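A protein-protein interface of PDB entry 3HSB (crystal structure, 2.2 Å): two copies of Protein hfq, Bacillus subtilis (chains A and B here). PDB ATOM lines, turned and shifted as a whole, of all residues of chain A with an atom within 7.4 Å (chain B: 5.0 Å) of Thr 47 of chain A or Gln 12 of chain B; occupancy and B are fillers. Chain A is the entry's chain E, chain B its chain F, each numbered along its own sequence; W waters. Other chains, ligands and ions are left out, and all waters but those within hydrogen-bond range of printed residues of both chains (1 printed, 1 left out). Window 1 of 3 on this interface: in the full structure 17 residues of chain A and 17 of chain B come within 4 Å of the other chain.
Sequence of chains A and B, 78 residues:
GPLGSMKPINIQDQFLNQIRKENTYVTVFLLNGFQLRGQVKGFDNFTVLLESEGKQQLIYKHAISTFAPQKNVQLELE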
ATOM      1  N   GLN A  12      -7.398  31.502 -16.986  1.00  0.00           N
ATOM      2  CA  GLN A  12      -8.842  31.390 -16.901  1.00  0.00           C
ATOM      3  C   GLN A  12      -9.390  31.782 -15.517  1.00  0.00           C
ATOM      4  O   GLN A  12     -10.345  32.575 -15.394  1.00  0.00           O
ATOM      5  CB  GLN A  12      -9.282  29.984 -17.270  1.00  0.00           C
ATOM      6  CG  GLN A  12     -10.763  29.796 -17.124  1.00  0.00           C
ATOM      7  CD  GLN A  12     -11.200  28.372 -17.396  1.00  0.00           C
ATOM      8  OE1 GLN A  12     -12.373  28.127 -17.387  1.00  0.00           O
ATOM      9  NE2 GLN A  12     -10.248  27.424 -17.630  1.00  0.00           N
ATOM     10  N   LEU A  16     -11.760  34.946 -14.300  1.00  0.00           N
ATOM     11  CA  LEU A  16     -13.069  34.699 -13.739  1.00  0.00           C
ATOM     12  C   LEU A  16     -13.066  35.133 -12.251  1.00  0.00           C
ATOM     13  O   LEU A  16     -14.008  35.698 -11.796  1.00  0.00           O
ATOM     14  CB  LEU A  16     -13.459  33.198 -13.846  1.00  0.00           C
ATOM     15  CG  LEU A  16     -13.798  32.670 -15.283  1.00  0.00           C
ATOM     16  CD1 LEU A  16     -14.094  31.159 -15.368  1.00  0.00           C
ATOM     17  CD2 LEU A  16     -14.923  33.461 -15.876  1.00  0.00           C
ATOM     18  N   GLY A  42     -19.943  32.801  -9.567  1.00  0.00           N
ATOM     19  CA  GLY A  42     -19.172  31.647  -9.089  1.00  0.00           C
ATOM     20  C   GLY A  42     -18.850  30.786 -10.298  1.00  0.00           C
ATOM     21  O   GLY A  42     -19.432  30.994 -11.371  1.00  0.00           O
ATOM     22  N   PHE A  43     -17.937  29.828 -10.119  1.00  0.00           N
ATOM     23  CA  PHE A  43     -17.556  28.907 -11.181  1.00  0.00           C
ATOM     24  C   PHE A  43     -16.827  27.768 -10.563  1.00  0.00           C
ATOM     25  O   PHE A  43     -16.211  27.887  -9.482  1.00  0.00           O
ATOM     26  CB  PHE A  43     -16.643  29.581 -12.188  1.00  0.00           C
ATOM     27  CG  PHE A  43     -15.407  30.187 -11.601  1.00  0.00           C
ATOM     28  CD1 PHE A  43     -14.184  29.506 -11.665  1.00  0.00           C
ATOM     29  CD2 PHE A  43     -15.444  31.437 -11.018  1.00  0.00           C
ATOM     30  CE1 PHE A  43     -13.013  30.059 -11.164  1.00  0.00           C
ATOM     31  CE2 PHE A  43     -14.258  31.987 -10.467  1.00  0.00           C
ATOM     32  CZ  PHE A  43     -13.041  31.275 -10.563  1.00  0.00           C
ATOM     33  N   ASP A  44     -16.841  26.656 -11.257  1.00  0.00           N
ATOM     34  CA  ASP A  44     -15.990  25.556 -10.849  1.00  0.00           C
ATOM     35  C   ASP A  44     -15.230  25.089 -12.126  1.00  0.00           C
ATOM     36  O   ASP A  44     -15.187  25.811 -13.102  1.00  0.00           O
ATOM     37  CB  ASP A  44     -16.864  24.494 -10.077  1.00  0.00           C
ATOM     38  CG  ASP A  44     -17.964  23.836 -10.947  1.00  0.00           C
ATOM     39  OD1 ASP A  44     -17.964  24.017 -12.137  1.00  0.00           O
ATOM     40  OD2 ASP A  44     -18.828  23.095 -10.475  1.00  0.00           O
ATOM     41  N   ASN A  45     -14.721  23.871 -12.177  1.00  0.00           N
ATOM     42  CA  ASN A  45     -14.077  23.327 -13.412  1.00  0.00           C
ATOM     43  C   ASN A  45     -14.922  23.128 -14.715  1.00  0.00           C
ATOM     44  O   ASN A  45     -14.349  23.111 -15.813  1.00  0.00           O
ATOM     45  CB  ASN A  45     -13.467  21.946 -13.168  1.00  0.00           C
ATOM     46  CG  ASN A  45     -12.468  21.909 -12.075  1.00  0.00           C
ATOM     47  OD1 ASN A  45     -11.696  22.879 -11.813  1.00  0.00           O
ATOM     48  ND2 ASN A  45     -12.415  20.751 -11.435  1.00  0.00           N
ATOM     49  N   PHE A  46     -16.225  22.923 -14.576  1.00  0.00           N
ATOM     50  CA  PHE A  46     -17.135  22.684 -15.692  1.00  0.00           C
ATOM     51  C   PHE A  46     -18.153  23.780 -16.024  1.00  0.00           C
ATOM     52  O   PHE A  46     -18.680  23.808 -17.156  1.00  0.00           O
ATOM     53  CB  PHE A  46     -17.818  21.324 -15.454  1.00  0.00           C
ATOM     54  CG  PHE A  46     -16.816  20.203 -15.402  1.00  0.00           C
ATOM     55  CD1 PHE A  46     -16.485  19.587 -14.191  1.00  0.00           C
ATOM     56  CD2 PHE A  46     -16.164  19.802 -16.567  1.00  0.00           C
ATOM     57  CE1 PHE A  46     -15.505  18.546 -14.171  1.00  0.00           C
ATOM     58  CE2 PHE A  46     -15.177  18.755 -16.559  1.00  0.00           C
ATOM     59  CZ  PHE A  46     -14.853  18.157 -15.382  1.00  0.00           C
ATOM     60  N   THR A  47     -18.415  24.678 -15.052  1.00  0.00           N
ATOM     61  CA  THR A  47     -19.497  25.593 -15.185  1.00  0.00           C
ATOM     62  C   THR A  47     -19.173  27.022 -14.678  1.00  0.00           C
ATOM     63  O   THR A  47     -18.220  27.246 -13.932  1.00  0.00           O
ATOM     64  CB  THR A  47     -20.737  25.134 -14.440  1.00  0.00           C
ATOM     65  OG1 THR A  47     -20.484  25.193 -13.017  1.00  0.00           O
ATOM     66  CG2 THR A  47     -21.201  23.729 -14.889  1.00  0.00           C
ATOM     67  N   VAL A  48     -19.931  27.993 -15.186  1.00  0.00           N
ATOM     68  CA  VAL A  48     -19.871  29.366 -14.674  1.00  0.00           C
ATOM     69  C   VAL A  48     -21.317  29.687 -14.253  1.00  0.00           C
ATOM     70  O   VAL A  48     -22.260  29.494 -15.061  1.00  0.00           O
ATOM     71  CB  VAL A  48     -19.376  30.298 -15.784  1.00  0.00           C
ATOM     72  CG1 VAL A  48     -19.427  31.673 -15.345  1.00  0.00           C
ATOM     73  CG2 VAL A  48     -17.935  29.934 -16.183  1.00  0.00           C
ATOM     74  N   LEU A  49     -21.499  30.122 -13.004  1.00  0.00           N
ATOM     75  CA  LEU A  49     -22.776  30.733 -12.537  1.00  0.00           C
ATOM     76  C   LEU A  49     -22.797  32.228 -12.811  1.00  0.00           C
ATOM     77  O   LEU A  49     -22.021  32.970 -12.263  1.00  0.00           O
ATOM     78  CB  LEU A  49     -23.015  30.505 -11.040  1.00  0.00           C
ATOM     79  CG  LEU A  49     -24.407  30.893 -10.486  1.00  0.00           C
ATOM     80  CD1 LEU A  49     -25.565  30.119 -11.181  1.00  0.00           C
ATOM     81  CD2 LEU A  49     -24.381  30.581  -9.026  1.00  0.00           C
ATOM     82  N   LEU A  50     -23.687  32.639 -13.702  1.00  0.00           N
ATOM     83  CA  LEU A  50     -23.820  33.993 -14.121  1.00  0.00           C
ATOM     84  C   LEU A  50     -25.195  34.540 -13.572  1.00  0.00           C
ATOM     85  O   LEU A  50     -26.145  33.784 -13.333  1.00  0.00           O
ATOM     86  CB  LEU A  50     -23.766  34.058 -15.667  1.00  0.00           C
ATOM     87  CG  LEU A  50     -23.619  35.419 -16.336  1.00  0.00           C
ATOM     88  CD1 LEU A  50     -22.182  35.926 -16.337  1.00  0.00           C
ATOM     89  CD2 LEU A  50     -24.131  35.384 -17.710  1.00  0.00           C
ATOM     90  N   LEU A  58     -26.856  28.828 -14.865  1.00  0.00           N
ATOM     91  CA  LEU A  58     -25.706  27.934 -14.793  1.00  0.00           C
ATOM     92  C   LEU A  58     -25.339  27.561 -16.238  1.00  0.00           C
ATOM     93  O   LEU A  58     -26.123  26.913 -16.939  1.00  0.00           O
ATOM     94  CB  LEU A  58     -26.032  26.672 -14.000  1.00  0.00           C
ATOM     95  CG  LEU A  58     -24.762  25.873 -13.649  1.00  0.00           C
ATOM     96  CD1 LEU A  58     -23.817  26.593 -12.637  1.00  0.00           C
ATOM     97  CD2 LEU A  58     -25.070  24.455 -13.163  1.00  0.00           C
ATOM     98  N   ILE A  59     -24.151  27.957 -16.661  1.00  0.00           N
ATOM     99  CA  ILE A  59     -23.703  27.819 -18.059  1.00  0.00           C
ATOM    100  C   ILE A  59     -22.540  26.809 -18.076  1.00  0.00           C
ATOM    101  O   ILE A  59     -21.609  26.954 -17.285  1.00  0.00           O
ATOM    102  CB  ILE A  59     -23.074  29.132 -18.567  1.00  0.00           C
ATOM    103  CG1 ILE A  59     -24.058  30.309 -18.301  1.00  0.00           C
ATOM    104  CG2 ILE A  59     -22.707  28.990 -20.062  1.00  0.00           C
ATOM    105  CD1 ILE A  59     -23.404  31.602 -18.520  1.00  0.00           C
ATOM    106  N   TYR A  60     -22.566  25.832 -18.979  1.00  0.00           N
ATOM    107  CA  TYR A  60     -21.448  24.912 -19.089  1.00  0.00           C
ATOM    108  C   TYR A  60     -20.316  25.600 -19.808  1.00  0.00           C
ATOM    109  O   TYR A  60     -20.475  26.140 -20.896  1.00  0.00           O
ATOM    110  CB  TYR A  60     -21.835  23.632 -19.845  1.00  0.00           C
ATOM    111  CG  TYR A  60     -22.578  22.643 -18.956  1.00  0.00           C
ATOM    112  CD1 TYR A  60     -21.915  21.976 -17.942  1.00  0.00           C
ATOM    113  CD2 TYR A  60     -23.945  22.539 -19.011  1.00  0.00           C
ATOM    114  CE1 TYR A  60     -22.591  21.140 -17.049  1.00  0.00           C
ATOM    115  CE2 TYR A  60     -24.624  21.669 -18.176  1.00  0.00           C
ATOM    116  CZ  TYR A  60     -23.912  20.976 -17.173  1.00  0.00           C
ATOM    117  OH  TYR A  60     -24.532  20.124 -16.282  1.00  0.00           O
ATOM    118  N   LYS A  61     -19.130  25.515 -19.259  1.00  0.00           N
ATOM    119  CA  LYS A  61     -17.996  26.040 -20.052  1.00  0.00           C
ATOM    120  C   LYS A  61     -17.914  25.467 -21.456  1.00  0.00           C
ATOM    121  O   LYS A  61     -17.547  26.220 -22.373  1.00  0.00           O
ATOM    122  CB  LYS A  61     -16.647  25.809 -19.334  1.00  0.00           C
ATOM    123  CG  LYS A  61     -16.512  26.590 -18.086  1.00  0.00           C
ATOM    124  CD  LYS A  61     -15.191  26.147 -17.365  1.00  0.00           C
ATOM    125  CE  LYS A  61     -15.074  26.952 -16.063  1.00  0.00           C
ATOM    126  NZ  LYS A  61     -13.769  26.898 -15.403  1.00  0.00           N
ATOM    127  N   HIS A  62     -18.155  24.141 -21.663  1.00  0.00           N
ATOM    128  CA  HIS A  62     -18.126  23.585 -23.047  1.00  0.00           C
ATOM    129  C   HIS A  62     -19.006  24.345 -23.989  1.00  0.00           C
ATOM    130  O   HIS A  62     -18.801  24.231 -25.198  1.00  0.00           O
ATOM    131  CB  HIS A  62     -18.482  22.040 -23.154  1.00  0.00           C
ATOM    132  CG  HIS A  62     -19.875  21.668 -22.666  1.00  0.00           C
ATOM    133  ND1 HIS A  62     -20.094  20.963 -21.513  1.00  0.00           N
ATOM    134  CD2 HIS A  62     -21.102  21.930 -23.177  1.00  0.00           C
ATOM    135  CE1 HIS A  62     -21.394  20.770 -21.345  1.00  0.00           C
ATOM    136  NE2 HIS A  62     -22.024  21.409 -22.310  1.00  0.00           N
ATOM    137  N   ILE A  64     -19.458  27.681 -24.112  1.00  0.00           N
ATOM    138  CA  ILE A  64     -19.022  29.059 -24.209  1.00  0.00           C
ATOM    139  C   ILE A  64     -17.880  29.204 -25.214  1.00  0.00           C
ATOM    140  O   ILE A  64     -16.939  28.330 -25.257  1.00  0.00           O
ATOM    141  CB  ILE A  64     -18.538  29.598 -22.811  1.00  0.00           C
ATOM    142  CG1 ILE A  64     -19.701  29.617 -21.773  1.00  0.00           C
ATOM    143  CG2 ILE A  64     -17.886  31.048 -22.998  1.00  0.00           C
ATOM    144  CD1 ILE A  64     -19.216  30.009 -20.275  1.00  0.00           C
ATOM    145  N   ASN B  10     -18.688  22.185  -5.003  1.00  0.00           N
ATOM    146  CA  ASN B  10     -18.864  22.132  -6.497  1.00  0.00           C
ATOM    147  C   ASN B  10     -20.162  22.904  -6.826  1.00  0.00           C
ATOM    148  O   ASN B  10     -21.230  22.542  -6.423  1.00  0.00           O
ATOM    149  CB  ASN B  10     -18.917  20.670  -6.862  1.00  0.00           C
ATOM    150  CG  ASN B  10     -19.378  20.399  -8.260  1.00  0.00           C
ATOM    151  OD1 ASN B  10     -20.519  20.642  -8.567  1.00  0.00           O
ATOM    152  ND2 ASN B  10     -18.541  19.740  -9.069  1.00  0.00           N
ATOM    153  N   ILE B  11     -20.040  23.964  -7.592  1.00  0.00           N
ATOM    154  CA  ILE B  11     -21.153  24.818  -7.969  1.00  0.00           C
ATOM    155  C   ILE B  11     -22.182  24.024  -8.773  1.00  0.00           C
ATOM    156  O   ILE B  11     -23.373  24.014  -8.449  1.00  0.00           O
ATOM    157  CB  ILE B  11     -20.560  26.132  -8.654  1.00  0.00           C
ATOM    158  CG1 ILE B  11     -20.094  27.077  -7.554  1.00  0.00           C
ATOM    159  CG2 ILE B  11     -21.525  26.793  -9.547  1.00  0.00           C
ATOM    160  CD1 ILE B  11     -20.508  28.590  -7.736  1.00  0.00           C
ATOM    161  N   GLN B  12     -21.731  23.207  -9.708  1.00  0.00           N
ATOM    162  CA  GLN B  12     -22.702  22.498 -10.631  1.00  0.00           C
ATOM    163  C   GLN B  12     -23.587  21.548  -9.827  1.00  0.00           C
ATOM    164  O   GLN B  12     -24.825  21.453 -10.020  1.00  0.00           O
ATOM    165  CB  GLN B  12     -21.911  21.688 -11.704  1.00  0.00           C
ATOM    166  CG  GLN B  12     -22.813  20.924 -12.643  1.00  0.00           C
ATOM    167  CD  GLN B  12     -22.062  19.985 -13.574  1.00  0.00           C
ATOM    168  OE1 GLN B  12     -20.832  19.911 -13.553  1.00  0.00           O
ATOM    169  NE2 GLN B  12     -22.805  19.256 -14.386  1.00  0.00           N
ATOM    170  N   ASP B  13     -22.934  20.767  -8.981  1.00  0.00           N
ATOM    171  CA  ASP B  13     -23.613  19.789  -8.143  1.00  0.00           C
ATOM    172  C   ASP B  13     -24.567  20.341  -7.070  1.00  0.00           C
ATOM    173  O   ASP B  13     -25.645  19.776  -6.828  1.00  0.00           O
ATOM    174  CB  ASP B  13     -22.577  18.861  -7.498  1.00  0.00           C
ATOM    175  CG  ASP B  13     -22.043  17.811  -8.479  1.00  0.00           C
ATOM    176  OD1 ASP B  13     -21.464  16.816  -8.008  1.00  0.00           O
ATOM    177  OD2 ASP B  13     -22.213  17.910  -9.726  1.00  0.00           O
ATOM    178  N   GLN B  14     -24.165  21.402  -6.414  1.00  0.00           N
ATOM    179  CA  GLN B  14     -25.091  22.186  -5.590  1.00  0.00           C
ATOM    180  C   GLN B  14     -26.312  22.688  -6.302  1.00  0.00           C
ATOM    181  O   GLN B  14     -27.447  22.527  -5.811  1.00  0.00           O
ATOM    182  CB  GLN B  14     -24.374  23.436  -5.043  1.00  0.00           C
ATOM    183  CG  GLN B  14     -23.393  23.118  -3.971  1.00  0.00           C
ATOM    184  CD  GLN B  14     -22.799  24.374  -3.426  1.00  0.00           C
ATOM    185  OE1 GLN B  14     -23.519  25.193  -2.890  1.00  0.00           O
ATOM    186  NE2 GLN B  14     -21.471  24.552  -3.591  1.00  0.00           N
ATOM    187  N   PHE B  15     -26.093  23.357  -7.430  1.00  0.00           N
ATOM    188  CA  PHE B  15     -27.175  23.898  -8.261  1.00  0.00           C
ATOM    189  C   PHE B  15     -28.153  22.823  -8.656  1.00  0.00           C
ATOM    190  O   PHE B  15     -29.373  22.943  -8.370  1.00  0.00           O
ATOM    191  CB  PHE B  15     -26.580  24.640  -9.469  1.00  0.00           C
ATOM    192  CG  PHE B  15     -27.604  25.268 -10.377  1.00  0.00           C
ATOM    193  CD1 PHE B  15     -27.894  26.613 -10.263  1.00  0.00           C
ATOM    194  CD2 PHE B  15     -28.277  24.494 -11.379  1.00  0.00           C
ATOM    195  CE1 PHE B  15     -28.857  27.230 -11.098  1.00  0.00           C
ATOM    196  CE2 PHE B  15     -29.203  25.096 -12.289  1.00  0.00           C
ATOM    197  CZ  PHE B  15     -29.469  26.498 -12.141  1.00  0.00           C
ATOM    198  N   LEU B  16     -27.652  21.712  -9.233  1.00  0.00           N
ATOM    199  CA  LEU B  16     -28.529  20.684  -9.714  1.00  0.00           C
ATOM    200  C   LEU B  16     -29.240  19.998  -8.551  1.00  0.00           C
ATOM    201  O   LEU B  16     -30.417  19.618  -8.662  1.00  0.00           O
ATOM    202  CB  LEU B  16     -27.746  19.653 -10.559  1.00  0.00           C
ATOM    203  CG  LEU B  16     -27.276  20.136 -11.960  1.00  0.00           C
ATOM    204  CD1 LEU B  16     -26.275  19.147 -12.608  1.00  0.00           C
ATOM    205  CD2 LEU B  16     -28.504  20.395 -12.898  1.00  0.00           C
ATOM    206  N   ASN B  17     -28.553  19.816  -7.432  1.00  0.00           N
ATOM    207  CA  ASN B  17     -29.206  19.142  -6.363  1.00  0.00           C
ATOM    208  C   ASN B  17     -30.259  20.051  -5.720  1.00  0.00           C
ATOM    209  O   ASN B  17     -31.293  19.589  -5.311  1.00  0.00           O
ATOM    210  CB  ASN B  17     -28.207  18.768  -5.278  1.00  0.00           C
ATOM    211  CG  ASN B  17     -28.768  17.726  -4.352  1.00  0.00           C
ATOM    212  OD1 ASN B  17     -29.127  16.637  -4.795  1.00  0.00           O
ATOM    213  ND2 ASN B  17     -28.898  18.065  -3.086  1.00  0.00           N
ATOM    214  N   LYS B  61     -25.229  16.122 -20.591  1.00  0.00           N
ATOM    215  CA  LYS B  61     -24.741  17.488 -20.235  1.00  0.00           C
ATOM    216  C   LYS B  61     -23.944  18.112 -21.366  1.00  0.00           C
ATOM    217  O   LYS B  61     -24.010  19.310 -21.541  1.00  0.00           O
ATOM    218  CB  LYS B  61     -23.834  17.342 -19.016  1.00  0.00           C
ATOM    219  CG  LYS B  61     -24.598  17.089 -17.748  1.00  0.00           C
ATOM    220  CD  LYS B  61     -23.501  16.871 -16.664  1.00  0.00           C
ATOM    221  CE  LYS B  61     -24.167  16.739 -15.311  1.00  0.00           C
ATOM    222  NZ  LYS B  61     -23.125  16.628 -14.304  1.00  0.00           N
HETATM  223  O   HOH W   1     -18.642  20.826 -11.758  1.00  0.00           O
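Positions printed for both chains: 12, 16 and 61.
Water W1 lies within hydrogen-bond range of the side-chain carboxylate (OD2) of Asp 44 of chain A (2.6 Å), the side-chain amide nitrogen (ND2) of Asn 10 of chain B (2.9 Å) and the side-chain amide oxygen (OE1) of Gln 12 of chain B (3.0 Å).
Thr 47 of chain A touches two residues of chain B. Of the printed residues of chain B, Tyr 60 of chain A touches Gln 12 (2.7 Å) and Lys 61 (3.4 Å). Printed residues of chain B within 4 Å of Asp 44 of chain A: Asn 10 (3.5 Å), Ile 11 (3.2 Å) and Gln 12 (3.0 Å). The nearest printed residue of chain B that does not touch Thr 47 of chain A is Asn 10 of chain B (6.4 Å). The nearest printed residue of chain A that does not touch Gln 12 of chain B is Phe 43 of chain A (6.8 Å). The nearest printed residue of chain B that does not touch Asp 44 of chain A is Asp 13 of chain B (5.0 Å).
OD2 of Asp 44 of chain A sits at hydrogen-bond distance from N of Ile 11 of chain B (3.2 Å). OD2 of Asp 44 of chain A sits at hydrogen-bond distance from N of Gln 12 of chain B (3.0 Å). NE2 of Gln 12 of chain B is in hydrogen-bond range of OH of Tyr 60 of chain A (2.7 Å). A ring nitrogen (NE2) of His 62 of chain A is in hydrogen-bond range of the backbone carbonyl oxygen (O) of Lys 61 of chain B (3.0 Å).
Hydrophobic or aromatic side chains of chain B that line the printed part of chain A: Ile 11 and Phe 15. Along chain B the printed residues that touch a printed residue of chain A span positions 10 to 61. Of the 17 printed residues of chain A, 8 touch a printed residue of chain B. Among the printed residues, no Asp or Glu carboxylate lies within 4 Å of a Lys or Arg side-chain nitrogen of the other chain.
CD1 of Ile 11 of chain B touches CA of Gly 42 of chain A, at 3.6 Å. Phe 43 of chain A touches Ile 11 of chain B (N to CD1, 3.7 Å). Asp 44 of chain A touches Asn 10 of chain B. Gln 12 of chain B touches Phe 46 of chain A. OG1 of Thr 47 of chain A touches CG2 of Ile 11 of chain B (3.96 Å). CG2 of Thr 47 of chain A touches CB of Gln 12 of chain B (3.8 Å). Ile 11 of chain B touches Leu 58 of chain A (CG2 to CD1, 3.9 Å). Gln 12 of chain B touches Leu 58 of chain A (CA to CD2, 3.98 Å). Phe 15 of chain B touches Leu 58 of chain A (CD2 to CD2, 3.7 Å). Lys 61 of chain B touches Tyr 60 of chain A (CG to OH, 3.4 Å).
OD1 of Asp 44 of chain A sits at hydrogen-bond distance from N of Phe 46 of chain A, 3.2 Å away. O of Asp 44 of chain A lies within hydrogen-bond range of NZ of Lys 61 of chain A (2.9 Å). N of Gln 12 of chain B lies within hydrogen-bond range of OD1 of Asn 10 of chain B (3.1 Å). The side-chain amide oxygen (OD1) of Asn 10 of chain B is in hydrogen-bond range of the backbone NH (N) of Asp 13 of chain B (2.5 Å). The side-chain amide nitrogen of Gln 14 of chain B lies close to the backbone carbonyl oxygen of Asn 10 of chain B, 3.5 Å away. The side-chain amide nitrogen (NE2) of Gln 12 of chain B lies close to the side-chain amino group (NZ) of Lys 61 of chain B (2.6 Å).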
